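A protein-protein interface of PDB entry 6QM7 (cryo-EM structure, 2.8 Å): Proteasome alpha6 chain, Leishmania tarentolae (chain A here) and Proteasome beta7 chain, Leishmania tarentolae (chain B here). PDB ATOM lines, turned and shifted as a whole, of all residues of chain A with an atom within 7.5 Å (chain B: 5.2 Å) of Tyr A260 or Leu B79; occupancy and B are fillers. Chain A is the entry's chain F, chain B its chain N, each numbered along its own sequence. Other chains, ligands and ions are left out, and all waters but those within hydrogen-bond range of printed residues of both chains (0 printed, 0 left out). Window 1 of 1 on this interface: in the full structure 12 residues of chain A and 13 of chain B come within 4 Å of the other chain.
ND2 of Asn B66 lies within hydrogen-bond range of OH of Tyr A264, 2.5 Å away.
OH of Tyr A260 is in hydrogen-bond range of NE2 of Gln B70, at 2.7 Å.
The side-chain amide nitrogen (NE2) of Gln B70 sits at hydrogen-bond distance from the side-chain amide oxygen (OE1) of Gln A272 (2.8 Å).
The side-chain amide nitrogen (ND2) of Asn A266 is in hydrogen-bond range of the side-chain carboxylate (OE2) of Glu B83 (3.3 Å).
Among the printed residues, merely in contact across the chains: Tyr A264 with Glu B83 (3.3 Å), Tyr A260 with Leu B79 (3.5 Å) and Tyr A264 with Leu B79 (3.5 Å).
Of chain B, only Gln B70 (2.7 Å) and Leu B79 (3.5 Å) come within 4 Å of Tyr A260.
Of the printed residues of chain A, Leu B79 touches Tyr A260 and Tyr A264.
Of the printed residues of chain B, Asn A266 touches Glu B83 (3.3 Å).
Of the printed residues of chain B, Tyr A264 touches Asn B66 (2.5 Å), Leu B79 (3.5 Å) and Glu B83 (3.3 Å).
Printed residues of chain A within 4 Å of Gln B70: Tyr A260 (2.7 Å) and Gln A272 (2.8 Å).
Met A268 touches none of the printed residues of chain B.
Thr A255 touches none of the printed residues of chain B.
The nearest residue of chain A that does not touch Leu B79 is Pro A269 (6.3 Å).
Hydrophobic or aromatic side chains of chain B that line the printed part of chain A: Leu B79.
Of the 21 printed residues of chain A, 4 touch a printed residue of chain B.
Among the printed residues, no Asp or Glu carboxylate lies within 4 Å of a Lys or Arg side-chain nitrogen of the other chain.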
ATOM      1  N   ASP A 232       4.515 -25.671 -21.766  1.00  0.00           N
ATOM      2  CA  ASP A 232       5.300 -25.073 -20.661  1.00  0.00           C
ATOM      3  C   ASP A 232       4.416 -24.010 -20.024  1.00  0.00           C
ATOM      4  O   ASP A 232       3.339 -23.763 -20.567  1.00  0.00           O
ATOM      5  CB  ASP A 232       6.627 -24.506 -21.177  1.00  0.00           C
ATOM      6  CG  ASP A 232       7.747 -24.423 -20.148  1.00  0.00           C
ATOM      7  OD1 ASP A 232       8.569 -23.487 -20.259  1.00  0.00           O
ATOM      8  OD2 ASP A 232       7.829 -25.323 -19.275  1.00  0.00           O
ATOM      9  N   HIS A 234       4.229 -21.049 -20.321  1.00  0.00           N
ATOM     10  CA  HIS A 234       3.939 -19.905 -21.222  1.00  0.00           C
ATOM     11  C   HIS A 234       3.422 -20.347 -22.591  1.00  0.00           C
ATOM     12  O   HIS A 234       3.234 -19.462 -23.420  1.00  0.00           O
ATOM     13  CB  HIS A 234       5.200 -19.057 -21.388  1.00  0.00           C
ATOM     14  CG  HIS A 234       6.261 -19.694 -22.221  1.00  0.00           C
ATOM     15  ND1 HIS A 234       6.921 -20.836 -21.828  1.00  0.00           N
ATOM     16  CD2 HIS A 234       6.793 -19.344 -23.416  1.00  0.00           C
ATOM     17  CE1 HIS A 234       7.802 -21.176 -22.749  1.00  0.00           C
ATOM     18  NE2 HIS A 234       7.754 -20.277 -23.726  1.00  0.00           N
ATOM     19  N   ARG A 254       7.436 -30.179 -25.587  1.00  0.00           N
ATOM     20  CA  ARG A 254       7.605 -30.237 -24.114  1.00  0.00           C
ATOM     21  C   ARG A 254       9.074 -30.451 -23.800  1.00  0.00           C
ATOM     22  O   ARG A 254       9.611 -29.704 -22.994  1.00  0.00           O
ATOM     23  CB  ARG A 254       6.763 -31.353 -23.497  1.00  0.00           C
ATOM     24  CG  ARG A 254       5.318 -30.937 -23.296  1.00  0.00           C
ATOM     25  CD  ARG A 254       4.414 -32.129 -23.162  1.00  0.00           C
ATOM     26  NE  ARG A 254       3.090 -31.707 -22.747  1.00  0.00           N
ATOM     27  CZ  ARG A 254       2.078 -32.527 -22.596  1.00  0.00           C
ATOM     28  NH1 ARG A 254       2.232 -33.821 -22.821  1.00  0.00           N
ATOM     29  NH2 ARG A 254       0.917 -32.055 -22.204  1.00  0.00           N
ATOM     30  N   THR A 255       9.674 -31.439 -24.444  1.00  0.00           N
ATOM     31  CA  THR A 255      11.096 -31.809 -24.273  1.00  0.00           C
ATOM     32  C   THR A 255      11.976 -30.612 -24.618  1.00  0.00           C
ATOM     33  O   THR A 255      12.907 -30.336 -23.843  1.00  0.00           O
ATOM     34  CB  THR A 255      11.457 -33.007 -25.145  1.00  0.00           C
ATOM     35  OG1 THR A 255      10.546 -34.054 -24.809  1.00  0.00           O
ATOM     36  CG2 THR A 255      12.890 -33.437 -24.943  1.00  0.00           C
ATOM     37  N   GLU A 256      11.687 -29.936 -25.731  1.00  0.00           N
ATOM     38  CA  GLU A 256      12.500 -28.798 -26.228  1.00  0.00           C
ATOM     39  C   GLU A 256      12.290 -27.592 -25.312  1.00  0.00           C
ATOM     40  O   GLU A 256      13.294 -26.904 -25.022  1.00  0.00           O
ATOM     41  CB  GLU A 256      12.173 -28.470 -27.688  1.00  0.00           C
ATOM     42  CG  GLU A 256      12.702 -29.495 -28.685  1.00  0.00           C
ATOM     43  CD  GLU A 256      14.192 -29.818 -28.611  1.00  0.00           C
ATOM     44  OE1 GLU A 256      14.997 -28.887 -28.360  1.00  0.00           O
ATOM     45  OE2 GLU A 256      14.546 -31.013 -28.794  1.00  0.00           O
ATOM     46  N   CYS A 257      11.059 -27.354 -24.863  1.00  0.00           N
ATOM     47  CA  CYS A 257      10.731 -26.224 -23.956  1.00  0.00           C
ATOM     48  C   CYS A 257      11.400 -26.421 -22.603  1.00  0.00           C
ATOM     49  O   CYS A 257      11.815 -25.411 -22.015  1.00  0.00           O
ATOM     50  CB  CYS A 257       9.232 -26.013 -23.809  1.00  0.00           C
ATOM     51  SG  CYS A 257       8.554 -25.228 -25.297  1.00  0.00           S
ATOM     52  N   MET A 258      11.513 -27.669 -22.158  1.00  0.00           N
ATOM     53  CA  MET A 258      12.190 -28.020 -20.891  1.00  0.00           C
ATOM     54  C   MET A 258      13.680 -27.749 -21.047  1.00  0.00           C
ATOM     55  O   MET A 258      14.214 -27.016 -20.208  1.00  0.00           O
ATOM     56  CB  MET A 258      11.971 -29.487 -20.524  1.00  0.00           C
ATOM     57  CG  MET A 258      10.635 -29.719 -19.878  1.00  0.00           C
ATOM     58  SD  MET A 258      10.433 -31.423 -19.374  1.00  0.00           S
ATOM     59  CE  MET A 258       8.656 -31.575 -19.547  1.00  0.00           C
ATOM     60  N   ASN A 259      14.300 -28.350 -22.066  1.00  0.00           N
ATOM     61  CA  ASN A 259      15.718 -28.124 -22.437  1.00  0.00           C
ATOM     62  C   ASN A 259      16.021 -26.631 -22.416  1.00  0.00           C
ATOM     63  O   ASN A 259      16.992 -26.232 -21.760  1.00  0.00           O
ATOM     64  CB  ASN A 259      16.032 -28.634 -23.834  1.00  0.00           C
ATOM     65  CG  ASN A 259      16.502 -30.063 -23.803  1.00  0.00           C
ATOM     66  OD1 ASN A 259      17.601 -30.314 -23.315  1.00  0.00           O
ATOM     67  ND2 ASN A 259      15.686 -30.990 -24.294  1.00  0.00           N
ATOM     68  N   TYR A 260      15.224 -25.843 -23.129  1.00  0.00           N
ATOM     69  CA  TYR A 260      15.433 -24.384 -23.227  1.00  0.00           C
ATOM     70  C   TYR A 260      15.440 -23.818 -21.820  1.00  0.00           C
ATOM     71  O   TYR A 260      16.446 -23.235 -21.423  1.00  0.00           O
ATOM     72  CB  TYR A 260      14.366 -23.703 -24.082  1.00  0.00           C
ATOM     73  CG  TYR A 260      14.690 -22.268 -24.369  1.00  0.00           C
ATOM     74  CD1 TYR A 260      15.321 -21.881 -25.535  1.00  0.00           C
ATOM     75  CD2 TYR A 260      14.416 -21.305 -23.426  1.00  0.00           C
ATOM     76  CE1 TYR A 260      15.657 -20.551 -25.752  1.00  0.00           C
ATOM     77  CE2 TYR A 260      14.730 -19.974 -23.627  1.00  0.00           C
ATOM     78  CZ  TYR A 260      15.364 -19.595 -24.792  1.00  0.00           C
ATOM     79  OH  TYR A 260      15.643 -18.273 -24.968  1.00  0.00           O
ATOM     80  N   ARG A 261      14.362 -24.036 -21.077  1.00  0.00           N
ATOM     81  CA  ARG A 261      14.181 -23.495 -19.705  1.00  0.00           C
ATOM     82  C   ARG A 261      15.283 -24.004 -18.770  1.00  0.00           C
ATOM     83  O   ARG A 261      15.716 -23.251 -17.913  1.00  0.00           O
ATOM     84  CB  ARG A 261      12.801 -23.868 -19.179  1.00  0.00           C
ATOM     85  CG  ARG A 261      12.418 -23.132 -17.909  1.00  0.00           C
ATOM     86  CD  ARG A 261      10.987 -23.423 -17.540  1.00  0.00           C
ATOM     87  NE  ARG A 261      10.060 -22.641 -18.351  1.00  0.00           N
ATOM     88  CZ  ARG A 261       9.803 -21.347 -18.191  1.00  0.00           C
ATOM     89  NH1 ARG A 261      10.433 -20.645 -17.258  1.00  0.00           N
ATOM     90  NH2 ARG A 261       8.913 -20.757 -18.973  1.00  0.00           N
ATOM     91  N   TYR A 262      15.727 -25.236 -18.919  1.00  0.00           N
ATOM     92  CA  TYR A 262      16.900 -25.754 -18.184  1.00  0.00           C
ATOM     93  C   TYR A 262      18.102 -24.859 -18.486  1.00  0.00           C
ATOM     94  O   TYR A 262      18.749 -24.358 -17.527  1.00  0.00           O
ATOM     95  CB  TYR A 262      17.197 -27.206 -18.544  1.00  0.00           C
ATOM     96  CG  TYR A 262      18.513 -27.683 -18.004  1.00  0.00           C
ATOM     97  CD1 TYR A 262      18.716 -27.821 -16.643  1.00  0.00           C
ATOM     98  CD2 TYR A 262      19.577 -27.959 -18.848  1.00  0.00           C
ATOM     99  CE1 TYR A 262      19.937 -28.251 -16.140  1.00  0.00           C
ATOM    100  CE2 TYR A 262      20.802 -28.388 -18.358  1.00  0.00           C
ATOM    101  CZ  TYR A 262      20.981 -28.532 -17.001  1.00  0.00           C
ATOM    102  OH  TYR A 262      22.189 -28.923 -16.518  1.00  0.00           O
ATOM    103  N   MET A 263      18.385 -24.639 -19.769  1.00  0.00           N
ATOM    104  CA  MET A 263      19.581 -23.883 -20.207  1.00  0.00           C
ATOM    105  C   MET A 263      19.488 -22.432 -19.748  1.00  0.00           C
ATOM    106  O   MET A 263      20.436 -21.967 -19.111  1.00  0.00           O
ATOM    107  CB  MET A 263      19.748 -23.915 -21.725  1.00  0.00           C
ATOM    108  CG  MET A 263      20.361 -25.198 -22.202  1.00  0.00           C
ATOM    109  SD  MET A 263      22.073 -25.341 -21.645  1.00  0.00           S
ATOM    110  CE  MET A 263      22.161 -27.121 -21.458  1.00  0.00           C
ATOM    111  N   TYR A 264      18.384 -21.761 -20.049  1.00  0.00           N
ATOM    112  CA  TYR A 264      18.293 -20.287 -19.998  1.00  0.00           C
ATOM    113  C   TYR A 264      17.516 -19.796 -18.779  1.00  0.00           C
ATOM    114  O   TYR A 264      17.565 -18.587 -18.516  1.00  0.00           O
ATOM    115  CB  TYR A 264      17.685 -19.800 -21.306  1.00  0.00           C
ATOM    116  CG  TYR A 264      18.508 -20.193 -22.501  1.00  0.00           C
ATOM    117  CD1 TYR A 264      19.741 -19.618 -22.736  1.00  0.00           C
ATOM    118  CD2 TYR A 264      18.069 -21.152 -23.386  1.00  0.00           C
ATOM    119  CE1 TYR A 264      20.512 -19.976 -23.825  1.00  0.00           C
ATOM    120  CE2 TYR A 264      18.825 -21.523 -24.480  1.00  0.00           C
ATOM    121  CZ  TYR A 264      20.051 -20.932 -24.705  1.00  0.00           C
ATOM    122  OH  TYR A 264      20.795 -21.312 -25.784  1.00  0.00           O
ATOM    123  N   SER A 265      16.825 -20.672 -18.056  1.00  0.00           N
ATOM    124  CA  SER A 265      16.015 -20.297 -16.868  1.00  0.00           C
ATOM    125  C   SER A 265      14.906 -19.341 -17.298  1.00  0.00           C
ATOM    126  O   SER A 265      14.611 -18.412 -16.533  1.00  0.00           O
ATOM    127  CB  SER A 265      16.871 -19.683 -15.770  1.00  0.00           C
ATOM    128  OG  SER A 265      17.942 -20.547 -15.409  1.00  0.00           O
ATOM    129  N   ASN A 266      14.329 -19.557 -18.476  1.00  0.00           N
ATOM    130  CA  ASN A 266      13.287 -18.670 -19.049  1.00  0.00           C
ATOM    131  C   ASN A 266      12.600 -19.422 -20.185  1.00  0.00           C
ATOM    132  O   ASN A 266      13.255 -20.238 -20.804  1.00  0.00           O
ATOM    133  CB  ASN A 266      13.885 -17.345 -19.533  1.00  0.00           C
ATOM    134  CG  ASN A 266      12.823 -16.337 -19.919  1.00  0.00           C
ATOM    135  OD1 ASN A 266      11.968 -15.991 -19.105  1.00  0.00           O
ATOM    136  ND2 ASN A 266      12.850 -15.877 -21.164  1.00  0.00           N
ATOM    137  N   GLY A 267      11.323 -19.168 -20.438  1.00  0.00           N
ATOM    138  CA  GLY A 267      10.554 -19.932 -21.437  1.00  0.00           C
ATOM    139  C   GLY A 267      11.081 -19.733 -22.844  1.00  0.00           C
ATOM    140  O   GLY A 267      11.423 -18.598 -23.194  1.00  0.00           O
ATOM    141  N   MET A 268      11.140 -20.796 -23.640  1.00  0.00           N
ATOM    142  CA  MET A 268      11.502 -20.692 -25.075  1.00  0.00           C
ATOM    143  C   MET A 268      10.650 -19.593 -25.700  1.00  0.00           C
ATOM    144  O   MET A 268       9.426 -19.639 -25.608  1.00  0.00           O
ATOM    145  CB  MET A 268      11.264 -22.010 -25.817  1.00  0.00           C
ATOM    146  CG  MET A 268      11.634 -21.947 -27.299  1.00  0.00           C
ATOM    147  SD  MET A 268      12.595 -23.373 -27.840  1.00  0.00           S
ATOM    148  CE  MET A 268      11.330 -24.641 -27.833  1.00  0.00           C
ATOM    149  N   PRO A 269      11.258 -18.567 -26.332  1.00  0.00           N
ATOM    150  CA  PRO A 269      10.508 -17.579 -27.093  1.00  0.00           C
ATOM    151  C   PRO A 269       9.661 -18.259 -28.161  1.00  0.00           C
ATOM    152  O   PRO A 269      10.096 -19.220 -28.710  1.00  0.00           O
ATOM    153  CB  PRO A 269      11.556 -16.720 -27.794  1.00  0.00           C
ATOM    154  CG  PRO A 269      12.829 -16.942 -27.020  1.00  0.00           C
ATOM    155  CD  PRO A 269      12.695 -18.285 -26.331  1.00  0.00           C
ATOM    156  N   GLN A 272      10.929 -18.626 -31.812  1.00  0.00           N
ATOM    157  CA  GLN A 272      11.926 -19.729 -31.852  1.00  0.00           C
ATOM    158  C   GLN A 272      11.239 -21.100 -31.868  1.00  0.00           C
ATOM    159  O   GLN A 272      11.746 -22.013 -32.533  1.00  0.00           O
ATOM    160  CB  GLN A 272      12.868 -19.685 -30.649  1.00  0.00           C
ATOM    161  CG  GLN A 272      13.969 -20.732 -30.734  1.00  0.00           C
ATOM    162  CD  GLN A 272      15.051 -20.542 -29.708  1.00  0.00           C
ATOM    163  OE1 GLN A 272      15.262 -19.450 -29.184  1.00  0.00           O
ATOM    164  NE2 GLN A 272      15.731 -21.633 -29.392  1.00  0.00           N
ATOM    165  N   MET A 273      10.163 -21.247 -31.110  1.00  0.00           N
ATOM    166  CA  MET A 273       9.407 -22.512 -30.993  1.00  0.00           C
ATOM    167  C   MET A 273       8.690 -22.802 -32.311  1.00  0.00           C
ATOM    168  O   MET A 273       8.704 -23.954 -32.720  1.00  0.00           O
ATOM    169  CB  MET A 273       8.380 -22.412 -29.867  1.00  0.00           C
ATOM    170  CG  MET A 273       7.848 -23.758 -29.418  1.00  0.00           C
ATOM    171  SD  MET A 273       6.700 -23.545 -28.049  1.00  0.00           S
ATOM    172  CE  MET A 273       7.718 -22.556 -26.956  1.00  0.00           C
ATOM    173  N   MET A 276      11.053 -24.233 -34.687  1.00  0.00           N
ATOM    174  CA  MET A 276      11.395 -25.627 -34.296  1.00  0.00           C
ATOM    175  C   MET A 276      10.357 -26.605 -34.830  1.00  0.00           C
ATOM    176  O   MET A 276      10.780 -27.684 -35.249  1.00  0.00           O
ATOM    177  CB  MET A 276      11.473 -25.822 -32.780  1.00  0.00           C
ATOM    178  CG  MET A 276      12.820 -25.479 -32.194  1.00  0.00           C
ATOM    179  SD  MET A 276      13.069 -26.304 -30.599  1.00  0.00           S
ATOM    180  CE  MET A 276      14.626 -25.556 -30.100  1.00  0.00           C
ATOM    181  N   HIS B  44      24.123  -6.561 -23.516  1.00  0.00           N
ATOM    182  CA  HIS B  44      23.741  -6.184 -22.126  1.00  0.00           C
ATOM    183  C   HIS B  44      24.782  -6.623 -21.106  1.00  0.00           C
ATOM    184  O   HIS B  44      24.777  -6.068 -20.012  1.00  0.00           O
ATOM    185  CB  HIS B  44      22.380  -6.789 -21.776  1.00  0.00           C
ATOM    186  CG  HIS B  44      21.341  -6.419 -22.775  1.00  0.00           C
ATOM    187  ND1 HIS B  44      21.076  -5.087 -23.087  1.00  0.00           N
ATOM    188  CD2 HIS B  44      20.561  -7.184 -23.576  1.00  0.00           C
ATOM    189  CE1 HIS B  44      20.150  -5.046 -24.022  1.00  0.00           C
ATOM    190  NE2 HIS B  44      19.812  -6.324 -24.338  1.00  0.00           N
ATOM    191  N   ASN B  66      26.056 -18.444 -29.288  1.00  0.00           N
ATOM    192  CA  ASN B  66      24.699 -18.819 -28.821  1.00  0.00           C
ATOM    193  C   ASN B  66      23.799 -17.580 -28.785  1.00  0.00           C
ATOM    194  O   ASN B  66      22.679 -17.644 -29.316  1.00  0.00           O
ATOM    195  CB  ASN B  66      24.758 -19.473 -27.442  1.00  0.00           C
ATOM    196  CG  ASN B  66      23.510 -20.254 -27.115  1.00  0.00           C
ATOM    197  OD1 ASN B  66      23.350 -21.387 -27.563  1.00  0.00           O
ATOM    198  ND2 ASN B  66      22.624 -19.648 -26.342  1.00  0.00           N
ATOM    199  N   ILE B  67      24.281 -16.488 -28.192  1.00  0.00           N
ATOM    200  CA  ILE B  67      23.518 -15.217 -28.045  1.00  0.00           C
ATOM    201  C   ILE B  67      23.225 -14.647 -29.433  1.00  0.00           C
ATOM    202  O   ILE B  67      22.052 -14.284 -29.651  1.00  0.00           O
ATOM    203  CB  ILE B  67      24.269 -14.180 -27.195  1.00  0.00           C
ATOM    204  CG1 ILE B  67      24.528 -14.648 -25.762  1.00  0.00           C
ATOM    205  CG2 ILE B  67      23.527 -12.850 -27.215  1.00  0.00           C
ATOM    206  CD1 ILE B  67      25.567 -13.803 -25.020  1.00  0.00           C
ATOM    207  N   GLN B  70      20.881 -17.093 -31.849  1.00  0.00           N
ATOM    208  CA  GLN B  70      19.456 -17.098 -31.422  1.00  0.00           C
ATOM    209  C   GLN B  70      18.773 -15.809 -31.900  1.00  0.00           C
ATOM    210  O   GLN B  70      17.671 -15.906 -32.441  1.00  0.00           O
ATOM    211  CB  GLN B  70      19.343 -17.259 -29.904  1.00  0.00           C
ATOM    212  CG  GLN B  70      17.983 -17.774 -29.450  1.00  0.00           C
ATOM    213  CD  GLN B  70      17.433 -17.111 -28.206  1.00  0.00           C
ATOM    214  OE1 GLN B  70      17.625 -15.917 -27.959  1.00  0.00           O
ATOM    215  NE2 GLN B  70      16.698 -17.885 -27.424  1.00  0.00           N
ATOM    216  N   ASP B  77      13.709 -11.484 -29.010  1.00  0.00           N
ATOM    217  CA  ASP B  77      14.490 -10.572 -28.139  1.00  0.00           C
ATOM    218  C   ASP B  77      15.747 -11.318 -27.703  1.00  0.00           C
ATOM    219  O   ASP B  77      15.662 -12.518 -27.405  1.00  0.00           O
ATOM    220  CB  ASP B  77      13.678 -10.044 -26.953  1.00  0.00           C
ATOM    221  CG  ASP B  77      12.993  -8.717 -27.263  1.00  0.00           C
ATOM    222  OD1 ASP B  77      13.621  -7.661 -27.009  1.00  0.00           O
ATOM    223  OD2 ASP B  77      11.842  -8.743 -27.766  1.00  0.00           O
ATOM    224  N   GLU B  78      16.868 -10.610 -27.721  1.00  0.00           N
ATOM    225  CA  GLU B  78      18.188 -11.078 -27.247  1.00  0.00           C
ATOM    226  C   GLU B  78      18.034 -11.680 -25.851  1.00  0.00           C
ATOM    227  O   GLU B  78      17.198 -11.187 -25.096  1.00  0.00           O
ATOM    228  CB  GLU B  78      19.127  -9.874 -27.231  1.00  0.00           C
ATOM    229  CG  GLU B  78      20.568 -10.214 -26.928  1.00  0.00           C
ATOM    230  CD  GLU B  78      21.537  -9.070 -27.176  1.00  0.00           C
ATOM    231  OE1 GLU B  78      21.187  -8.131 -27.943  1.00  0.00           O
ATOM    232  OE2 GLU B  78      22.642  -9.112 -26.592  1.00  0.00           O
ATOM    233  N   LEU B  79      18.832 -12.694 -25.519  1.00  0.00           N
ATOM    234  CA  LEU B  79      18.891 -13.262 -24.149  1.00  0.00           C
ATOM    235  C   LEU B  79      19.230 -12.156 -23.141  1.00  0.00           C
ATOM    236  O   LEU B  79      20.174 -11.365 -23.394  1.00  0.00           O
ATOM    237  CB  LEU B  79      19.959 -14.354 -24.090  1.00  0.00           C
ATOM    238  CG  LEU B  79      19.646 -15.676 -24.788  1.00  0.00           C
ATOM    239  CD1 LEU B  79      20.846 -16.609 -24.701  1.00  0.00           C
ATOM    240  CD2 LEU B  79      18.423 -16.348 -24.185  1.00  0.00           C
ATOM    241  N   SER B  80      18.497 -12.133 -22.024  1.00  0.00           N
ATOM    242  CA  SER B  80      18.816 -11.354 -20.802  1.00  0.00           C
ATOM    243  C   SER B  80      20.166 -11.781 -20.244  1.00  0.00           C
ATOM    244  O   SER B  80      20.613 -12.906 -20.457  1.00  0.00           O
ATOM    245  CB  SER B  80      17.763 -11.525 -19.748  1.00  0.00           C
ATOM    246  OG  SER B  80      16.647 -10.688 -20.029  1.00  0.00           O
ATOM    247  N   PRO B  81      20.840 -10.886 -19.493  1.00  0.00           N
ATOM    248  CA  PRO B  81      21.966 -11.267 -18.657  1.00  0.00           C
ATOM    249  C   PRO B  81      21.701 -12.562 -17.891  1.00  0.00           C
ATOM    250  O   PRO B  81      22.477 -13.468 -18.053  1.00  0.00           O
ATOM    251  CB  PRO B  81      22.052 -10.091 -17.701  1.00  0.00           C
ATOM    252  CG  PRO B  81      21.684  -8.927 -18.556  1.00  0.00           C
ATOM    253  CD  PRO B  81      20.572  -9.445 -19.442  1.00  0.00           C
ATOM    254  N   GLU B  83      19.735 -14.987 -18.393  1.00  0.00           N
ATOM    255  CA  GLU B  83      19.573 -16.141 -19.309  1.00  0.00           C
ATOM    256  C   GLU B  83      20.929 -16.519 -19.902  1.00  0.00           C
ATOM    257  O   GLU B  83      21.210 -17.711 -20.004  1.00  0.00           O
ATOM    258  CB  GLU B  83      18.556 -15.837 -20.408  1.00  0.00           C
ATOM    259  CG  GLU B  83      17.162 -15.486 -19.908  1.00  0.00           C
ATOM    260  CD  GLU B  83      16.227 -14.914 -20.971  1.00  0.00           C
ATOM    261  OE1 GLU B  83      16.261 -15.407 -22.137  1.00  0.00           O
ATOM    262  OE2 GLU B  83      15.451 -13.977 -20.637  1.00  0.00           O
ATOM    263  N   VAL B  84      21.721 -15.528 -20.304  1.00  0.00           N
ATOM    264  CA  VAL B  84      23.109 -15.729 -20.808  1.00  0.00           C
ATOM    265  C   VAL B  84      23.934 -16.377 -19.708  1.00  0.00           C
ATOM    266  O   VAL B  84      24.695 -17.291 -20.003  1.00  0.00           O
ATOM    267  CB  VAL B  84      23.767 -14.411 -21.213  1.00  0.00           C
ATOM    268  CG1 VAL B  84      25.253 -14.608 -21.491  1.00  0.00           C
ATOM    269  CG2 VAL B  84      23.073 -13.796 -22.407  1.00  0.00           C
ATOM    270  N   ARG B 112      19.787  -5.202 -18.387  1.00  0.00           N
ATOM    271  CA  ARG B 112      18.756  -5.183 -19.447  1.00  0.00           C
ATOM    272  C   ARG B 112      18.057  -3.820 -19.406  1.00  0.00           C
ATOM    273  O   ARG B 112      18.248  -3.031 -20.365  1.00  0.00           O
ATOM    274  CB  ARG B 112      17.784  -6.347 -19.250  1.00  0.00           C
ATOM    275  CG  ARG B 112      16.640  -6.361 -20.252  1.00  0.00           C
ATOM    276  CD  ARG B 112      17.054  -6.921 -21.589  1.00  0.00           C
ATOM    277  NE  ARG B 112      16.436  -8.220 -21.806  1.00  0.00           N
ATOM    278  CZ  ARG B 112      16.473  -8.896 -22.952  1.00  0.00           C
ATOM    279  NH1 ARG B 112      15.866 -10.070 -23.031  1.00  0.00           N
ATOM    280  NH2 ARG B 112      17.109  -8.412 -24.011  1.00  0.00           N
